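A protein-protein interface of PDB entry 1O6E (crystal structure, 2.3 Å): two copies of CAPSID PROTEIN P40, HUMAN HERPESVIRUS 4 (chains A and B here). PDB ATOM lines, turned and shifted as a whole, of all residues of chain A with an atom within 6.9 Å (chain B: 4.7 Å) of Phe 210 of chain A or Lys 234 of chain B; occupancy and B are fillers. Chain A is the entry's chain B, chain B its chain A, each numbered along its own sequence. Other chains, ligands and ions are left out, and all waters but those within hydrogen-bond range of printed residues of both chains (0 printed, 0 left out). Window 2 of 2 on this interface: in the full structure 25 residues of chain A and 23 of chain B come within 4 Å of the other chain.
No position is printed for both chains. Of the 8 pairs that touch across the chains among the printed residues, none has its exchanged pair printed and touching as well.
The side-chain carboxylate of Asp 207 of chain A sits at hydrogen-bond distance from the backbone NH of Ile 91 of chain B, 2.7 Å away.
Of the 8 printed residues of chain A, 4 touch a printed residue of chain B. Printed residues of chain A that touch a printed residue of chain B: Ile 206, Asp 207, Gly 209 and Phe 210. Along chain A the printed residues that touch a printed residue of chain B span positions 206 to 210.
Phe 210 of chain A touches five residues of chain B. Lys 234 of chain B touches one residue of chain A. Printed residues of chain A within 4 Å of Arg 214 of chain B: Gly 209 (3.4 Å) and Phe 210 (3.7 Å). Of the printed residues of chain B, Asp 207 of chain A touches Ile 91. Printed residues of chain A within 4 Å of Ala 110 of chain B: Ile 206 and Phe 210. Leu 211 of chain A touches none of the printed residues of chain B. The nearest residue of chain A that does not touch Lys 234 of chain B is Arg 212 of chain A (6.8 Å). The nearest printed residue of chain A that does not touch Val 215 of chain B is Arg 212 of chain A (4.1 Å).
NZ of Lys 234 of chain B lies within salt-bridge range of OE1 of Glu 106 of chain B, at 3.4 Å. The side-chain amino group (NZ) of Lys 234 of chain B is in hydrogen-bond range of the backbone carbonyl oxygen (O) of Ser 94 of chain B (3.2 Å). NZ of Lys 234 of chain B lies within hydrogen-bond range of O of Ala 92 of chain B.
Ile 206 of chain A touches Ala 110 of chain B. Gly 209 of chain A touches Arg 214 of chain B (O to CD, 3.4 Å). Ile 91 of chain B touches Phe 210 of chain A (CD1 to CB, 3.7 Å). Phe 210 of chain A touches Ala 110 of chain B (CE1 to O, 3.1 Å). CE1 of Phe 210 of chain A touches NH1 of Arg 214 of chain B, at 3.7 Å. Phe 210 of chain A touches Val 215 of chain B (CA to CG2, 3.5 Å). Phe 210 of chain A touches Lys 234 of chain B.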
ATOM      1  N   ALA A 205     -13.336  28.680   7.120  1.00  0.00           N
ATOM      2  CA  ALA A 205     -12.538  27.741   6.334  1.00  0.00           C
ATOM      3  C   ALA A 205     -13.426  27.075   5.292  1.00  0.00           C
ATOM      4  O   ALA A 205     -12.959  26.697   4.217  1.00  0.00           O
ATOM      5  CB  ALA A 205     -11.908  26.674   7.248  1.00  0.00           C
ATOM      6  N   ILE A 206     -14.705  26.927   5.628  1.00  0.00           N
ATOM      7  CA  ILE A 206     -15.670  26.320   4.716  1.00  0.00           C
ATOM      8  C   ILE A 206     -15.912  27.258   3.537  1.00  0.00           C
ATOM      9  O   ILE A 206     -15.980  26.818   2.391  1.00  0.00           O
ATOM     10  CB  ILE A 206     -17.025  26.019   5.418  1.00  0.00           C
ATOM     11  CG1 ILE A 206     -16.795  25.130   6.639  1.00  0.00           C
ATOM     12  CG2 ILE A 206     -17.975  25.319   4.449  1.00  0.00           C
ATOM     13  CD1 ILE A 206     -15.986  23.907   6.330  1.00  0.00           C
ATOM     14  N   ASP A 207     -16.034  28.553   3.825  1.00  0.00           N
ATOM     15  CA  ASP A 207     -16.260  29.550   2.785  1.00  0.00           C
ATOM     16  C   ASP A 207     -15.112  29.505   1.786  1.00  0.00           C
ATOM     17  O   ASP A 207     -15.307  29.730   0.581  1.00  0.00           O
ATOM     18  CB  ASP A 207     -16.357  30.973   3.382  1.00  0.00           C
ATOM     19  CG  ASP A 207     -17.686  31.234   4.108  1.00  0.00           C
ATOM     20  OD1 ASP A 207     -18.702  30.601   3.756  1.00  0.00           O
ATOM     21  OD2 ASP A 207     -17.719  32.096   5.020  1.00  0.00           O
ATOM     22  N   ALA A 208     -13.921  29.197   2.298  1.00  0.00           N
ATOM     23  CA  ALA A 208     -12.714  29.135   1.483  1.00  0.00           C
ATOM     24  C   ALA A 208     -12.624  27.866   0.648  1.00  0.00           C
ATOM     25  O   ALA A 208     -11.603  27.606   0.014  1.00  0.00           O
ATOM     26  CB  ALA A 208     -11.486  29.269   2.370  1.00  0.00           C
ATOM     27  N   GLY A 209     -13.690  27.076   0.661  1.00  0.00           N
ATOM     28  CA  GLY A 209     -13.718  25.859  -0.122  1.00  0.00           C
ATOM     29  C   GLY A 209     -14.411  26.125  -1.449  1.00  0.00           C
ATOM     30  O   GLY A 209     -14.253  25.358  -2.405  1.00  0.00           O
ATOM     31  N   PHE A 210     -15.168  27.224  -1.506  1.00  0.00           N
ATOM     32  CA  PHE A 210     -15.910  27.606  -2.705  1.00  0.00           C
ATOM     33  C   PHE A 210     -15.323  28.770  -3.484  1.00  0.00           C
ATOM     34  O   PHE A 210     -16.042  29.507  -4.156  1.00  0.00           O
ATOM     35  CB  PHE A 210     -17.365  27.901  -2.341  1.00  0.00           C
ATOM     36  CG  PHE A 210     -18.171  26.668  -2.085  1.00  0.00           C
ATOM     37  CD1 PHE A 210     -17.992  25.938  -0.918  1.00  0.00           C
ATOM     38  CD2 PHE A 210     -19.032  26.174  -3.060  1.00  0.00           C
ATOM     39  CE1 PHE A 210     -18.655  24.731  -0.726  1.00  0.00           C
ATOM     40  CE2 PHE A 210     -19.698  24.969  -2.883  1.00  0.00           C
ATOM     41  CZ  PHE A 210     -19.509  24.244  -1.720  1.00  0.00           C
ATOM     42  N   LEU A 211     -14.008  28.923  -3.399  1.00  0.00           N
ATOM     43  CA  LEU A 211     -13.304  29.988  -4.104  1.00  0.00           C
ATOM     44  C   LEU A 211     -12.782  29.473  -5.440  1.00  0.00           C
ATOM     45  O   LEU A 211     -11.790  28.739  -5.488  1.00  0.00           O
ATOM     46  CB  LEU A 211     -12.123  30.491  -3.268  1.00  0.00           C
ATOM     47  CG  LEU A 211     -12.425  31.143  -1.922  1.00  0.00           C
ATOM     48  CD1 LEU A 211     -11.131  31.474  -1.194  1.00  0.00           C
ATOM     49  CD2 LEU A 211     -13.232  32.398  -2.163  1.00  0.00           C
ATOM     50  N   ARG A 212     -13.448  29.859  -6.521  1.00  0.00           N
ATOM     51  CA  ARG A 212     -13.039  29.448  -7.858  1.00  0.00           C
ATOM     52  C   ARG A 212     -11.718  30.127  -8.244  1.00  0.00           C
ATOM     53  O   ARG A 212     -11.593  31.354  -8.177  1.00  0.00           O
ATOM     54  CB  ARG A 212     -14.115  29.829  -8.879  1.00  0.00           C
ATOM     55  CG  ARG A 212     -15.501  29.268  -8.598  1.00  0.00           C
ATOM     56  CD  ARG A 212     -16.522  29.868  -9.565  1.00  0.00           C
ATOM     57  NE  ARG A 212     -17.889  29.411  -9.306  1.00  0.00           N
ATOM     58  CZ  ARG A 212     -18.975  29.905  -9.899  1.00  0.00           C
ATOM     59  NH1 ARG A 212     -18.871  30.884 -10.794  1.00  0.00           N
ATOM     60  NH2 ARG A 212     -20.169  29.414  -9.597  1.00  0.00           N
ATOM     61  N   ILE B  91     -21.246  31.108   2.861  1.00  0.00           N
ATOM     62  CA  ILE B  91     -21.510  30.154   1.771  1.00  0.00           C
ATOM     63  C   ILE B  91     -22.687  29.244   2.103  1.00  0.00           C
ATOM     64  O   ILE B  91     -23.405  28.805   1.206  1.00  0.00           O
ATOM     65  CB  ILE B  91     -20.260  29.264   1.443  1.00  0.00           C
ATOM     66  CG1 ILE B  91     -19.437  29.892   0.302  1.00  0.00           C
ATOM     67  CG2 ILE B  91     -20.695  27.842   1.084  1.00  0.00           C
ATOM     68  CD1 ILE B  91     -20.133  29.908  -1.043  1.00  0.00           C
ATOM     69  N   ALA B  92     -22.874  28.961   3.389  1.00  0.00           N
ATOM     70  CA  ALA B  92     -23.980  28.125   3.844  1.00  0.00           C
ATOM     71  C   ALA B  92     -25.279  28.948   3.779  1.00  0.00           C
ATOM     72  O   ALA B  92     -26.286  28.509   3.205  1.00  0.00           O
ATOM     73  CB  ALA B  92     -23.719  27.637   5.278  1.00  0.00           C
ATOM     74  N   SER B  94     -25.993  31.768   2.093  1.00  0.00           N
ATOM     75  CA  SER B  94     -26.386  32.120   0.733  1.00  0.00           C
ATOM     76  C   SER B  94     -26.726  30.884  -0.089  1.00  0.00           C
ATOM     77  O   SER B  94     -25.976  29.910  -0.111  1.00  0.00           O
ATOM     78  CB  SER B  94     -25.261  32.878   0.038  1.00  0.00           C
ATOM     79  OG  SER B  94     -24.200  31.994  -0.276  1.00  0.00           O
ATOM     80  N   GLN B  95     -27.858  30.936  -0.775  1.00  0.00           N
ATOM     81  CA  GLN B  95     -28.296  29.832  -1.603  1.00  0.00           C
ATOM     82  C   GLN B  95     -28.031  30.133  -3.080  1.00  0.00           C
ATOM     83  O   GLN B  95     -28.017  31.293  -3.498  1.00  0.00           O
ATOM     84  CB  GLN B  95     -29.785  29.576  -1.363  1.00  0.00           C
ATOM     85  CG  GLN B  95     -30.094  29.192   0.069  1.00  0.00           C
ATOM     86  CD  GLN B  95     -31.570  29.252   0.404  1.00  0.00           C
ATOM     87  OE1 GLN B  95     -32.201  30.300   0.303  1.00  0.00           O
ATOM     88  NE2 GLN B  95     -32.125  28.125   0.815  1.00  0.00           N
ATOM     89  N   ARG B  96     -27.805  29.073  -3.855  1.00  0.00           N
ATOM     90  CA  ARG B  96     -27.540  29.171  -5.291  1.00  0.00           C
ATOM     91  C   ARG B  96     -28.846  29.531  -6.015  1.00  0.00           C
ATOM     92  O   ARG B  96     -28.849  30.274  -7.005  1.00  0.00           O
ATOM     93  CB  ARG B  96     -26.963  27.831  -5.779  1.00  0.00           C
ATOM     94  CG  ARG B  96     -26.799  27.672  -7.280  1.00  0.00           C
ATOM     95  CD  ARG B  96     -26.040  26.387  -7.606  1.00  0.00           C
ATOM     96  NE  ARG B  96     -26.595  25.181  -6.973  1.00  0.00           N
ATOM     97  CZ  ARG B  96     -27.682  24.524  -7.383  1.00  0.00           C
ATOM     98  NH1 ARG B  96     -28.363  24.947  -8.441  1.00  0.00           N
ATOM     99  NH2 ARG B  96     -28.083  23.431  -6.740  1.00  0.00           N
ATOM    100  N   GLU B 106     -27.877  23.177   5.012  1.00  0.00           N
ATOM    101  CA  GLU B 106     -27.158  24.106   4.147  1.00  0.00           C
ATOM    102  C   GLU B 106     -25.681  24.013   4.487  1.00  0.00           C
ATOM    103  O   GLU B 106     -24.821  24.141   3.614  1.00  0.00           O
ATOM    104  CB  GLU B 106     -27.615  25.560   4.382  1.00  0.00           C
ATOM    105  CG  GLU B 106     -29.127  25.848   4.269  1.00  0.00           C
ATOM    106  CD  GLU B 106     -29.546  26.457   2.941  1.00  0.00           C
ATOM    107  OE1 GLU B 106     -29.678  25.704   1.956  1.00  0.00           O
ATOM    108  OE2 GLU B 106     -29.742  27.690   2.883  1.00  0.00           O
ATOM    109  N   HIS B 109     -24.039  20.774   3.076  1.00  0.00           N
ATOM    110  CA  HIS B 109     -23.729  20.905   1.659  1.00  0.00           C
ATOM    111  C   HIS B 109     -22.556  21.803   1.276  1.00  0.00           C
ATOM    112  O   HIS B 109     -22.044  21.700   0.161  1.00  0.00           O
ATOM    113  CB  HIS B 109     -24.974  21.346   0.891  1.00  0.00           C
ATOM    114  CG  HIS B 109     -25.915  20.225   0.586  1.00  0.00           C
ATOM    115  ND1 HIS B 109     -26.727  19.653   1.540  1.00  0.00           N
ATOM    116  CD2 HIS B 109     -26.154  19.555  -0.565  1.00  0.00           C
ATOM    117  CE1 HIS B 109     -27.427  18.677   0.989  1.00  0.00           C
ATOM    118  NE2 HIS B 109     -27.097  18.597  -0.288  1.00  0.00           N
ATOM    119  N   ALA B 110     -22.138  22.686   2.175  1.00  0.00           N
ATOM    120  CA  ALA B 110     -21.020  23.577   1.881  1.00  0.00           C
ATOM    121  C   ALA B 110     -19.747  23.043   2.517  1.00  0.00           C
ATOM    122  O   ALA B 110     -18.644  23.221   1.995  1.00  0.00           O
ATOM    123  CB  ALA B 110     -21.316  24.968   2.397  1.00  0.00           C
ATOM    124  N   ARG B 214     -13.090  22.627  -7.594  1.00  0.00           N
ATOM    125  CA  ARG B 214     -13.954  21.890  -6.672  1.00  0.00           C
ATOM    126  C   ARG B 214     -15.431  22.203  -6.892  1.00  0.00           C
ATOM    127  O   ARG B 214     -16.261  21.312  -7.020  1.00  0.00           O
ATOM    128  CB  ARG B 214     -13.604  22.213  -5.217  1.00  0.00           C
ATOM    129  CG  ARG B 214     -14.416  21.391  -4.210  1.00  0.00           C
ATOM    130  CD  ARG B 214     -14.492  22.042  -2.835  1.00  0.00           C
ATOM    131  NE  ARG B 214     -15.240  21.208  -1.897  1.00  0.00           N
ATOM    132  CZ  ARG B 214     -15.707  21.618  -0.718  1.00  0.00           C
ATOM    133  NH1 ARG B 214     -15.514  22.863  -0.298  1.00  0.00           N
ATOM    134  NH2 ARG B 214     -16.387  20.775   0.043  1.00  0.00           N
ATOM    135  N   VAL B 215     -15.749  23.489  -6.914  1.00  0.00           N
ATOM    136  CA  VAL B 215     -17.120  23.950  -7.109  1.00  0.00           C
ATOM    137  C   VAL B 215     -17.675  23.501  -8.468  1.00  0.00           C
ATOM    138  O   VAL B 215     -18.830  23.080  -8.578  1.00  0.00           O
ATOM    139  CB  VAL B 215     -17.192  25.507  -7.036  1.00  0.00           C
ATOM    140  CG1 VAL B 215     -18.628  25.976  -7.185  1.00  0.00           C
ATOM    141  CG2 VAL B 215     -16.599  25.999  -5.731  1.00  0.00           C
ATOM    142  N   TYR B 232     -30.627  21.420  -2.414  1.00  0.00           N
ATOM    143  CA  TYR B 232     -29.788  22.268  -1.556  1.00  0.00           C
ATOM    144  C   TYR B 232     -28.280  22.131  -1.757  1.00  0.00           C
ATOM    145  O   TYR B 232     -27.497  22.290  -0.817  1.00  0.00           O
ATOM    146  CB  TYR B 232     -30.130  22.042  -0.084  1.00  0.00           C
ATOM    147  CG  TYR B 232     -31.463  22.623   0.318  1.00  0.00           C
ATOM    148  CD1 TYR B 232     -31.705  23.994   0.223  1.00  0.00           C
ATOM    149  CD2 TYR B 232     -32.489  21.804   0.793  1.00  0.00           C
ATOM    150  CE1 TYR B 232     -32.942  24.535   0.592  1.00  0.00           C
ATOM    151  CE2 TYR B 232     -33.726  22.334   1.164  1.00  0.00           C
ATOM    152  CZ  TYR B 232     -33.946  23.695   1.063  1.00  0.00           C
ATOM    153  OH  TYR B 232     -35.160  24.211   1.444  1.00  0.00           O
ATOM    154  N   LEU B 233     -27.887  21.856  -2.997  1.00  0.00           N
ATOM    155  CA  LEU B 233     -26.484  21.702  -3.350  1.00  0.00           C
ATOM    156  C   LEU B 233     -25.883  23.079  -3.579  1.00  0.00           C
ATOM    157  O   LEU B 233     -26.342  23.829  -4.431  1.00  0.00           O
ATOM    158  CB  LEU B 233     -26.344  20.858  -4.622  1.00  0.00           C
ATOM    159  CG  LEU B 233     -27.168  19.567  -4.710  1.00  0.00           C
ATOM    160  CD1 LEU B 233     -26.747  18.815  -5.955  1.00  0.00           C
ATOM    161  CD2 LEU B 233     -26.977  18.696  -3.475  1.00  0.00           C
ATOM    162  N   LYS B 234     -24.846  23.394  -2.811  1.00  0.00           N
ATOM    163  CA  LYS B 234     -24.173  24.685  -2.893  1.00  0.00           C
ATOM    164  C   LYS B 234     -23.410  24.884  -4.189  1.00  0.00           C
ATOM    165  O   LYS B 234     -22.790  25.927  -4.392  1.00  0.00           O
ATOM    166  CB  LYS B 234     -23.217  24.856  -1.703  1.00  0.00           C
ATOM    167  CG  LYS B 234     -23.913  24.874  -0.345  1.00  0.00           C
ATOM    168  CD  LYS B 234     -24.984  25.950  -0.310  1.00  0.00           C
ATOM    169  CE  LYS B 234     -25.814  25.908   0.955  1.00  0.00           C
ATOM    170  NZ  LYS B 234     -26.755  27.065   1.026  1.00  0.00           N
ATOM    171  N   ALA B 235     -23.451  23.891  -5.068  1.00  0.00           N
ATOM    172  CA  ALA B 235     -22.742  23.999  -6.338  1.00  0.00           C
ATOM    173  C   ALA B 235     -23.533  23.364  -7.483  1.00  0.00           C
ATOM    174  O   ALA B 235     -23.748  24.060  -8.511  1.00  0.00           O
ATOM    175  CB  ALA B 235     -21.352  23.355  -6.221  1.00  0.00           C
ATOM    176  OXT ALA B 235     -23.917  22.178  -7.339  1.00  0.00           O
